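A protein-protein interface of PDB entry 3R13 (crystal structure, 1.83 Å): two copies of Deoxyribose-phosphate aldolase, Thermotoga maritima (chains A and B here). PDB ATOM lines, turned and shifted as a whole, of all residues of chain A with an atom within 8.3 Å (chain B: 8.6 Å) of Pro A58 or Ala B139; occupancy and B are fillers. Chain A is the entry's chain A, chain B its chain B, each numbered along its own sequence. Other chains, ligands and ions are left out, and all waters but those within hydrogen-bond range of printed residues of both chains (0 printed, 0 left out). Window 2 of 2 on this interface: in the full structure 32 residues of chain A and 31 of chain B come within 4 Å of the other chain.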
ATOM      1  N   PHE A  55     -18.879 -23.748  19.728  1.00  0.00           N
ATOM      2  CA  PHE A  55     -18.817 -23.916  21.188  1.00  0.00           C
ATOM      3  C   PHE A  55     -19.381 -25.260  21.723  1.00  0.00           C
ATOM      4  O   PHE A  55     -19.437 -25.452  22.935  1.00  0.00           O
ATOM      5  CB  PHE A  55     -19.501 -22.713  21.863  1.00  0.00           C
ATOM      6  CG  PHE A  55     -20.885 -22.441  21.350  1.00  0.00           C
ATOM      7  CD1 PHE A  55     -21.968 -23.187  21.825  1.00  0.00           C
ATOM      8  CD2 PHE A  55     -21.113 -21.463  20.392  1.00  0.00           C
ATOM      9  CE1 PHE A  55     -23.268 -22.952  21.336  1.00  0.00           C
ATOM     10  CE2 PHE A  55     -22.389 -21.231  19.880  1.00  0.00           C
ATOM     11  CZ  PHE A  55     -23.478 -21.968  20.354  1.00  0.00           C
ATOM     12  N   ALA A  56     -19.755 -26.200  20.848  1.00  0.00           N
ATOM     13  CA  ALA A  56     -20.243 -27.508  21.312  1.00  0.00           C
ATOM     14  C   ALA A  56     -19.129 -28.248  22.051  1.00  0.00           C
ATOM     15  O   ALA A  56     -17.992 -28.259  21.589  1.00  0.00           O
ATOM     16  CB  ALA A  56     -20.763 -28.403  20.122  1.00  0.00           C
ATOM     17  N   THR A  57     -19.487 -28.895  23.150  1.00  0.00           N
ATOM     18  CA  THR A  57     -18.575 -29.651  23.997  1.00  0.00           C
ATOM     19  C   THR A  57     -18.718 -31.167  23.736  1.00  0.00           C
ATOM     20  O   THR A  57     -19.677 -31.605  23.106  1.00  0.00           O
ATOM     21  CB  THR A  57     -18.907 -29.348  25.468  1.00  0.00           C
ATOM     22  OG1 THR A  57     -20.284 -29.711  25.703  1.00  0.00           O
ATOM     23  CG2 THR A  57     -18.700 -27.868  25.803  1.00  0.00           C
ATOM     24  N   PRO A  58     -17.771 -31.988  24.232  1.00  0.00           N
ATOM     25  CA  PRO A  58     -18.019 -33.412  24.177  1.00  0.00           C
ATOM     26  C   PRO A  58     -19.385 -33.830  24.787  1.00  0.00           C
ATOM     27  O   PRO A  58     -20.066 -34.677  24.249  1.00  0.00           O
ATOM     28  CB  PRO A  58     -16.856 -33.983  24.969  1.00  0.00           C
ATOM     29  CG  PRO A  58     -15.735 -33.021  24.725  1.00  0.00           C
ATOM     30  CD  PRO A  58     -16.429 -31.685  24.756  1.00  0.00           C
ATOM     31  N   ASP A  59     -19.795 -33.209  25.875  1.00  0.00           N
ATOM     32  CA  ASP A  59     -21.081 -33.550  26.490  1.00  0.00           C
ATOM     33  C   ASP A  59     -22.276 -33.253  25.584  1.00  0.00           C
ATOM     34  O   ASP A  59     -23.239 -34.000  25.551  1.00  0.00           O
ATOM     35  CB  ASP A  59     -21.244 -32.793  27.807  1.00  0.00           C
ATOM     36  CG  ASP A  59     -20.497 -33.459  28.965  1.00  0.00           C
ATOM     37  OD1 ASP A  59     -20.008 -34.597  28.815  1.00  0.00           O
ATOM     38  OD2 ASP A  59     -20.400 -32.820  30.033  1.00  0.00           O
ATOM     39  N   ASP A  60     -22.218 -32.149  24.854  1.00  0.00           N
ATOM     40  CA  ASP A  60     -23.223 -31.824  23.845  1.00  0.00           C
ATOM     41  C   ASP A  60     -23.317 -32.904  22.766  1.00  0.00           C
ATOM     42  O   ASP A  60     -24.412 -33.246  22.327  1.00  0.00           O
ATOM     43  CB  ASP A  60     -22.879 -30.500  23.171  1.00  0.00           C
ATOM     44  CG  ASP A  60     -23.012 -29.317  24.099  1.00  0.00           C
ATOM     45  OD1 ASP A  60     -23.824 -29.413  25.046  1.00  0.00           O
ATOM     46  OD2 ASP A  60     -22.327 -28.289  23.872  1.00  0.00           O
ATOM     47  N   ILE A  61     -22.173 -33.406  22.310  1.00  0.00           N
ATOM     48  CA  ILE A  61     -22.166 -34.451  21.280  1.00  0.00           C
ATOM     49  C   ILE A  61     -22.756 -35.746  21.804  1.00  0.00           C
ATOM     50  O   ILE A  61     -23.482 -36.463  21.071  1.00  0.00           O
ATOM     51  CB  ILE A  61     -20.744 -34.706  20.712  1.00  0.00           C
ATOM     52  CG1 ILE A  61     -20.212 -33.435  20.063  1.00  0.00           C
ATOM     53  CG2 ILE A  61     -20.742 -35.883  19.680  1.00  0.00           C
ATOM     54  CD1 ILE A  61     -21.073 -32.854  19.008  1.00  0.00           C
ATOM     55  N   LYS A  62     -22.430 -36.075  23.062  1.00  0.00           N
ATOM     56  CA  LYS A  62     -23.014 -37.259  23.681  1.00  0.00           C
ATOM     57  C   LYS A  62     -24.504 -37.093  23.734  1.00  0.00           C
ATOM     58  O   LYS A  62     -25.235 -38.029  23.438  1.00  0.00           O
ATOM     59  CB  LYS A  62     -22.440 -37.490  25.050  1.00  0.00           C
ATOM     60  CG  LYS A  62     -21.008 -37.980  24.973  1.00  0.00           C
ATOM     61  CD  LYS A  62     -20.401 -38.139  26.403  1.00  0.00           C
ATOM     62  CE  LYS A  62     -18.874 -38.224  26.333  1.00  0.00           C
ATOM     63  NZ  LYS A  62     -18.251 -38.414  27.665  1.00  0.00           N
ATOM     64  N   LYS A  63     -24.987 -35.891  24.054  1.00  0.00           N
ATOM     65  CA  LYS A  63     -26.445 -35.696  24.086  1.00  0.00           C
ATOM     66  C   LYS A  63     -27.069 -35.817  22.697  1.00  0.00           C
ATOM     67  O   LYS A  63     -28.117 -36.431  22.515  1.00  0.00           O
ATOM     68  CB  LYS A  63     -26.778 -34.354  24.746  1.00  0.00           C
ATOM     69  CG  LYS A  63     -28.233 -34.094  25.008  1.00  0.00           C
ATOM     70  CD  LYS A  63     -28.433 -32.726  25.697  1.00  0.00           C
ATOM     71  CE  LYS A  63     -29.650 -31.988  25.143  1.00  0.00           C
ATOM     72  NZ  LYS A  63     -29.891 -30.729  25.890  1.00  0.00           N
ATOM     73  N   LEU A  64     -26.398 -35.269  21.701  1.00  0.00           N
ATOM     74  CA  LEU A  64     -26.857 -35.355  20.320  1.00  0.00           C
ATOM     75  C   LEU A  64     -26.970 -36.809  19.861  1.00  0.00           C
ATOM     76  O   LEU A  64     -27.968 -37.211  19.242  1.00  0.00           O
ATOM     77  CB  LEU A  64     -25.871 -34.622  19.405  1.00  0.00           C
ATOM     78  CG  LEU A  64     -26.264 -34.437  17.913  1.00  0.00           C
ATOM     79  CD1 LEU A  64     -27.279 -33.305  17.788  1.00  0.00           C
ATOM     80  CD2 LEU A  64     -24.987 -34.152  17.077  1.00  0.00           C
ATOM     81  N   CYS A  65     -25.960 -37.616  20.167  1.00  0.00           N
ATOM     82  CA  CYS A  65     -26.001 -39.050  19.756  1.00  0.00           C
ATOM     83  C   CYS A  65     -27.117 -39.792  20.487  1.00  0.00           C
ATOM     84  O   CYS A  65     -27.834 -40.596  19.878  1.00  0.00           O
ATOM     85  CB  CYS A  65     -24.623 -39.707  19.935  1.00  0.00           C
ATOM     86  SG  CYS A  65     -23.341 -38.974  18.880  1.00  0.00           S
ATOM     87  N   CYS A  81     -13.634 -32.638  14.474  1.00  0.00           N
ATOM     88  CA  CYS A  81     -12.938 -32.986  15.694  1.00  0.00           C
ATOM     89  C   CYS A  81     -13.742 -33.989  16.528  1.00  0.00           C
ATOM     90  O   CYS A  81     -13.158 -34.691  17.354  1.00  0.00           O
ATOM     91  CB  CYS A  81     -12.597 -31.760  16.520  1.00  0.00           C
ATOM     92  SG  CYS A  81     -14.076 -30.861  17.135  1.00  0.00           S
ATOM     93  N   TYR A  82     -15.051 -34.082  16.308  1.00  0.00           N
ATOM     94  CA  TYR A  82     -15.883 -34.961  17.104  1.00  0.00           C
ATOM     95  C   TYR A  82     -16.337 -36.261  16.439  1.00  0.00           C
ATOM     96  O   TYR A  82     -17.144 -36.994  16.996  1.00  0.00           O
ATOM     97  CB  TYR A  82     -17.088 -34.184  17.582  1.00  0.00           C
ATOM     98  CG  TYR A  82     -16.778 -33.121  18.619  1.00  0.00           C
ATOM     99  CD1 TYR A  82     -15.990 -33.401  19.735  1.00  0.00           C
ATOM    100  CD2 TYR A  82     -17.325 -31.858  18.512  1.00  0.00           C
ATOM    101  CE1 TYR A  82     -15.755 -32.439  20.694  1.00  0.00           C
ATOM    102  CE2 TYR A  82     -17.079 -30.876  19.467  1.00  0.00           C
ATOM    103  CZ  TYR A  82     -16.317 -31.182  20.569  1.00  0.00           C
ATOM    104  OH  TYR A  82     -16.111 -30.203  21.545  1.00  0.00           O
ATOM    105  N   LEU A  85     -15.481 -39.428  18.659  1.00  0.00           N
ATOM    106  CA  LEU A  85     -16.434 -39.462  19.777  1.00  0.00           C
ATOM    107  C   LEU A  85     -17.819 -39.951  19.352  1.00  0.00           C
ATOM    108  O   LEU A  85     -18.382 -40.855  19.992  1.00  0.00           O
ATOM    109  CB  LEU A  85     -16.518 -38.071  20.460  1.00  0.00           C
ATOM    110  CG  LEU A  85     -17.562 -37.905  21.580  1.00  0.00           C
ATOM    111  CD1 LEU A  85     -17.290 -38.934  22.653  1.00  0.00           C
ATOM    112  CD2 LEU A  85     -17.610 -36.494  22.139  1.00  0.00           C
ATOM    113  N   ALA A  86     -18.360 -39.386  18.263  1.00  0.00           N
ATOM    114  CA  ALA A  86     -19.681 -39.787  17.750  1.00  0.00           C
ATOM    115  C   ALA A  86     -19.717 -41.272  17.370  1.00  0.00           C
ATOM    116  O   ALA A  86     -20.655 -41.958  17.699  1.00  0.00           O
ATOM    117  CB  ALA A  86     -20.159 -38.877  16.569  1.00  0.00           C
ATOM    118  N   GLU A  89     -19.871 -43.322  20.527  1.00  0.00           N
ATOM    119  CA  GLU A  89     -21.171 -43.198  21.190  1.00  0.00           C
ATOM    120  C   GLU A  89     -22.257 -43.993  20.475  1.00  0.00           C
ATOM    121  O   GLU A  89     -23.182 -44.459  21.117  1.00  0.00           O
ATOM    122  CB  GLU A  89     -21.618 -41.727  21.279  1.00  0.00           C
ATOM    123  CG  GLU A  89     -20.804 -40.840  22.244  1.00  0.00           C
ATOM    124  CD  GLU A  89     -20.834 -41.327  23.689  1.00  0.00           C
ATOM    125  OE1 GLU A  89     -21.948 -41.484  24.228  1.00  0.00           O
ATOM    126  OE2 GLU A  89     -19.741 -41.523  24.285  1.00  0.00           O
ATOM    127  N   HIS B  11      -1.524 -31.005  31.477  1.00  0.00           N
ATOM    128  CA  HIS B  11      -2.845 -30.441  31.671  1.00  0.00           C
ATOM    129  C   HIS B  11      -2.913 -29.689  33.014  1.00  0.00           C
ATOM    130  O   HIS B  11      -3.390 -28.549  33.075  1.00  0.00           O
ATOM    131  CB  HIS B  11      -3.876 -31.565  31.611  1.00  0.00           C
ATOM    132  CG  HIS B  11      -5.292 -31.104  31.717  1.00  0.00           C
ATOM    133  ND1 HIS B  11      -5.879 -30.779  32.926  1.00  0.00           N
ATOM    134  CD2 HIS B  11      -6.246 -30.935  30.774  1.00  0.00           C
ATOM    135  CE1 HIS B  11      -7.125 -30.399  32.710  1.00  0.00           C
ATOM    136  NE2 HIS B  11      -7.373 -30.503  31.418  1.00  0.00           N
ATOM    137  N   ASN B 133     -10.070 -24.181  19.247  1.00  0.00           N
ATOM    138  CA  ASN B 133     -11.226 -25.053  19.434  1.00  0.00           C
ATOM    139  C   ASN B 133     -12.016 -24.600  20.670  1.00  0.00           C
ATOM    140  O   ASN B 133     -11.704 -24.967  21.824  1.00  0.00           O
ATOM    141  CB  ASN B 133     -10.820 -26.510  19.507  1.00  0.00           C
ATOM    142  CG  ASN B 133     -11.998 -27.440  19.396  1.00  0.00           C
ATOM    143  OD1 ASN B 133     -12.998 -27.254  20.057  1.00  0.00           O
ATOM    144  ND2 ASN B 133     -11.891 -28.436  18.531  1.00  0.00           N
ATOM    145  N   VAL B 134     -13.027 -23.777  20.407  1.00  0.00           N
ATOM    146  CA  VAL B 134     -13.822 -23.090  21.459  1.00  0.00           C
ATOM    147  C   VAL B 134     -14.528 -24.096  22.355  1.00  0.00           C
ATOM    148  O   VAL B 134     -14.549 -23.934  23.578  1.00  0.00           O
ATOM    149  CB  VAL B 134     -14.831 -22.111  20.814  1.00  0.00           C
ATOM    150  CG1 VAL B 134     -15.771 -21.430  21.824  1.00  0.00           C
ATOM    151  CG2 VAL B 134     -14.100 -21.071  19.970  1.00  0.00           C
ATOM    152  N   GLY B 135     -15.108 -25.140  21.759  1.00  0.00           N
ATOM    153  CA  GLY B 135     -15.853 -26.101  22.537  1.00  0.00           C
ATOM    154  C   GLY B 135     -14.960 -26.872  23.495  1.00  0.00           C
ATOM    155  O   GLY B 135     -15.341 -27.145  24.618  1.00  0.00           O
ATOM    156  N   MET B 136     -13.760 -27.231  23.055  1.00  0.00           N
ATOM    157  CA  MET B 136     -12.847 -27.920  23.958  1.00  0.00           C
ATOM    158  C   MET B 136     -12.320 -26.972  25.051  1.00  0.00           C
ATOM    159  O   MET B 136     -12.098 -27.392  26.198  1.00  0.00           O
ATOM    160  CB  MET B 136     -11.756 -28.598  23.175  1.00  0.00           C
ATOM    161  CG  MET B 136     -12.319 -29.692  22.275  1.00  0.00           C
ATOM    162  SD  MET B 136     -12.950 -31.169  23.345  1.00  0.00           S
ATOM    163  CE  MET B 136     -11.174 -31.877  23.804  1.00  0.00           C
ATOM    164  N   LEU B 137     -12.145 -25.703  24.729  1.00  0.00           N
ATOM    165  CA  LEU B 137     -11.816 -24.693  25.787  1.00  0.00           C
ATOM    166  C   LEU B 137     -12.948 -24.583  26.814  1.00  0.00           C
ATOM    167  O   LEU B 137     -12.710 -24.602  28.030  1.00  0.00           O
ATOM    168  CB  LEU B 137     -11.596 -23.325  25.164  1.00  0.00           C
ATOM    169  CG  LEU B 137     -11.070 -22.147  25.979  1.00  0.00           C
ATOM    170  CD1 LEU B 137      -9.542 -22.312  26.265  1.00  0.00           C
ATOM    171  CD2 LEU B 137     -11.303 -20.898  25.235  1.00  0.00           C
ATOM    172  N   LYS B 138     -14.177 -24.477  26.323  1.00  0.00           N
ATOM    173  CA  LYS B 138     -15.327 -24.398  27.214  1.00  0.00           C
ATOM    174  C   LYS B 138     -15.459 -25.669  28.058  1.00  0.00           C
ATOM    175  O   LYS B 138     -15.885 -25.591  29.200  1.00  0.00           O
ATOM    176  CB  LYS B 138     -16.622 -24.041  26.440  1.00  0.00           C
ATOM    177  CG  LYS B 138     -16.523 -22.578  25.888  1.00  0.00           C
ATOM    178  CD  LYS B 138     -17.835 -21.935  25.566  1.00  0.00           C
ATOM    179  CE  LYS B 138     -18.562 -21.472  26.784  1.00  0.00           C
ATOM    180  NZ  LYS B 138     -18.411 -20.007  27.053  1.00  0.00           N
ATOM    181  N   ALA B 139     -15.008 -26.810  27.549  1.00  0.00           N
ATOM    182  CA  ALA B 139     -14.970 -28.058  28.342  1.00  0.00           C
ATOM    183  C   ALA B 139     -13.744 -28.170  29.265  1.00  0.00           C
ATOM    184  O   ALA B 139     -13.583 -29.157  29.950  1.00  0.00           O
ATOM    185  CB  ALA B 139     -15.040 -29.265  27.419  1.00  0.00           C
ATOM    186  N   LYS B 140     -12.885 -27.150  29.278  1.00  0.00           N
ATOM    187  CA  LYS B 140     -11.710 -27.086  30.137  1.00  0.00           C
ATOM    188  C   LYS B 140     -10.699 -28.182  29.785  1.00  0.00           C
ATOM    189  O   LYS B 140      -9.957 -28.637  30.618  1.00  0.00           O
ATOM    190  CB  LYS B 140     -12.102 -27.130  31.626  1.00  0.00           C
ATOM    191  CG  LYS B 140     -13.083 -26.049  32.044  1.00  0.00           C
ATOM    192  CD  LYS B 140     -13.355 -26.124  33.568  1.00  0.00           C
ATOM    193  CE  LYS B 140     -13.992 -24.860  34.135  1.00  0.00           C
ATOM    194  NZ  LYS B 140     -14.631 -24.052  33.051  1.00  0.00           N
ATOM    195  N   GLU B 141     -10.688 -28.595  28.519  1.00  0.00           N
ATOM    196  CA  GLU B 141      -9.749 -29.574  28.003  1.00  0.00           C
ATOM    197  C   GLU B 141      -8.477 -28.865  27.573  1.00  0.00           C
ATOM    198  O   GLU B 141      -8.159 -28.790  26.388  1.00  0.00           O
ATOM    199  CB  GLU B 141     -10.382 -30.328  26.835  1.00  0.00           C
ATOM    200  CG  GLU B 141     -11.546 -31.225  27.248  1.00  0.00           C
ATOM    201  CD  GLU B 141     -11.120 -32.439  28.008  1.00  0.00           C
ATOM    202  OE1 GLU B 141      -9.925 -32.767  28.005  1.00  0.00           O
ATOM    203  OE2 GLU B 141     -11.981 -33.104  28.605  1.00  0.00           O
ATOM    204  N   TRP B 142      -7.747 -28.341  28.561  1.00  0.00           N
ATOM    205  CA  TRP B 142      -6.641 -27.424  28.309  1.00  0.00           C
ATOM    206  C   TRP B 142      -5.533 -28.073  27.472  1.00  0.00           C
ATOM    207  O   TRP B 142      -4.975 -27.465  26.561  1.00  0.00           O
ATOM    208  CB  TRP B 142      -5.992 -26.955  29.600  1.00  0.00           C
ATOM    209  CG  TRP B 142      -6.877 -26.393  30.653  1.00  0.00           C
ATOM    210  CD1 TRP B 142      -6.792 -26.670  32.005  1.00  0.00           C
ATOM    211  CD2 TRP B 142      -7.948 -25.462  30.504  1.00  0.00           C
ATOM    212  NE1 TRP B 142      -7.744 -25.983  32.685  1.00  0.00           N
ATOM    213  CE2 TRP B 142      -8.467 -25.223  31.805  1.00  0.00           C
ATOM    214  CE3 TRP B 142      -8.529 -24.805  29.415  1.00  0.00           C
ATOM    215  CZ2 TRP B 142      -9.527 -24.354  32.047  1.00  0.00           C
ATOM    216  CZ3 TRP B 142      -9.585 -23.915  29.670  1.00  0.00           C
ATOM    217  CH2 TRP B 142     -10.080 -23.722  30.980  1.00  0.00           C
ATOM    218  N   TYR B 144      -5.794 -30.616  25.266  1.00  0.00           N
ATOM    219  CA  TYR B 144      -6.255 -30.641  23.873  1.00  0.00           C
ATOM    220  C   TYR B 144      -6.046 -29.294  23.178  1.00  0.00           C
ATOM    221  O   TYR B 144      -5.471 -29.225  22.083  1.00  0.00           O
ATOM    222  CB  TYR B 144      -7.725 -31.048  23.759  1.00  0.00           C
ATOM    223  CG  TYR B 144      -8.167 -31.163  22.301  1.00  0.00           C
ATOM    224  CD1 TYR B 144      -8.574 -30.042  21.589  1.00  0.00           C
ATOM    225  CD2 TYR B 144      -8.128 -32.390  21.633  1.00  0.00           C
ATOM    226  CE1 TYR B 144      -8.968 -30.134  20.261  1.00  0.00           C
ATOM    227  CE2 TYR B 144      -8.499 -32.490  20.283  1.00  0.00           C
ATOM    228  CZ  TYR B 144      -8.934 -31.355  19.616  1.00  0.00           C
ATOM    229  OH  TYR B 144      -9.303 -31.394  18.298  1.00  0.00           O
ATOM    230  N   VAL B 145      -6.516 -28.220  23.807  1.00  0.00           N
ATOM    231  CA  VAL B 145      -6.429 -26.889  23.202  1.00  0.00           C
ATOM    232  C   VAL B 145      -4.945 -26.487  22.976  1.00  0.00           C
ATOM    233  O   VAL B 145      -4.567 -25.977  21.905  1.00  0.00           O
ATOM    234  CB  VAL B 145      -7.182 -25.847  24.063  1.00  0.00           C
ATOM    235  CG1 VAL B 145      -6.968 -24.399  23.525  1.00  0.00           C
ATOM    236  CG2 VAL B 145      -8.706 -26.262  24.152  1.00  0.00           C
ATOM    237  N   LEU B 170     -17.010 -16.475  24.894  1.00  0.00           N
ATOM    238  CA  LEU B 170     -16.248 -16.739  26.104  1.00  0.00           C
ATOM    239  C   LEU B 170     -16.579 -15.787  27.251  1.00  0.00           C
ATOM    240  O   LEU B 170     -16.791 -14.578  27.047  1.00  0.00           O
ATOM    241  CB  LEU B 170     -14.748 -16.590  25.801  1.00  0.00           C
ATOM    242  CG  LEU B 170     -14.110 -17.411  24.661  1.00  0.00           C
ATOM    243  CD1 LEU B 170     -12.561 -17.227  24.642  1.00  0.00           C
ATOM    244  CD2 LEU B 170     -14.478 -18.889  24.728  1.00  0.00           C
ATOM    245  N   GLU B 174     -12.396 -17.515  30.657  1.00  0.00           N
ATOM    246  CA  GLU B 174     -12.064 -18.267  29.446  1.00  0.00           C
ATOM    247  C   GLU B 174     -11.232 -17.421  28.482  1.00  0.00           C
ATOM    248  O   GLU B 174     -10.393 -17.926  27.768  1.00  0.00           O
ATOM    249  CB  GLU B 174     -13.347 -18.757  28.764  1.00  0.00           C
ATOM    250  CG  GLU B 174     -14.072 -19.831  29.533  1.00  0.00           C
ATOM    251  CD  GLU B 174     -15.511 -20.088  29.061  1.00  0.00           C
ATOM    252  OE1 GLU B 174     -16.167 -19.211  28.426  1.00  0.00           O
ATOM    253  OE2 GLU B 174     -15.977 -21.211  29.347  1.00  0.00           O
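The side-chain sulfur (SG) of Cys A81 sits at hydrogen-bond distance from the side-chain amide nitrogen (ND2) of Asn B133 (3.6 Å). The side-chain hydroxyl of Tyr A82 sits at hydrogen-bond distance from the side-chain sulfur of Met B136 (3.8 Å).
The backbone carbonyl oxygen of Ala A56 lies within hydrogen-bond range of the side-chain hydroxyl of Tyr A82 (2.7 Å). OD2 of Asp A60 lies within hydrogen-bond range of N of Thr A57, 3.0 Å away. OD1 of Asn B133 lies close to N of Gly B135 (3.4 Å). The backbone NH (N) of Met B136 is in hydrogen-bond range of the side-chain amide oxygen (OD1) of Asn B133, 3.1 Å away. The backbone NH (N) of Glu B141 sits at hydrogen-bond distance from the backbone carbonyl oxygen (O) of Met B136 (3.0 Å).
Phe A55 touches Val B134. Phe A55 touches Gly B135 (O to CA, 3.7 Å). Gly B135 touches Ala A56 (CA to O, 3.2 Å). CG2 of Thr A57 touches O of Gly B135 (3.6 Å). Pro A58 touches Met B136. Ala B139 touches Pro A58 (CB to CD, 3.9 Å). Tyr B144 touches Cys A81 (OH to CB, 3.8 Å).
Asp A60 touches none of the printed residues of chain B. Of the printed residues of chain B, Cys A81 touches Asn B133 (3.6 Å) and Tyr B144 (3.8 Å). Of the printed residues of chain A, Val B134 touches Phe A55. Ala B139 touches just one residue of chain A: Pro A58. Glu B141 touches none of the printed residues of chain A. The nearest printed residue of chain A that does not touch Asn B133 is Tyr A82 (4.5 Å).
Among the printed residues, 9 pairs touch across the chains. Among the printed residues, no Asp or Glu carboxylate lies within 4 Å of a Lys or Arg side-chain nitrogen of the other chain.
No position is printed for both chains.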
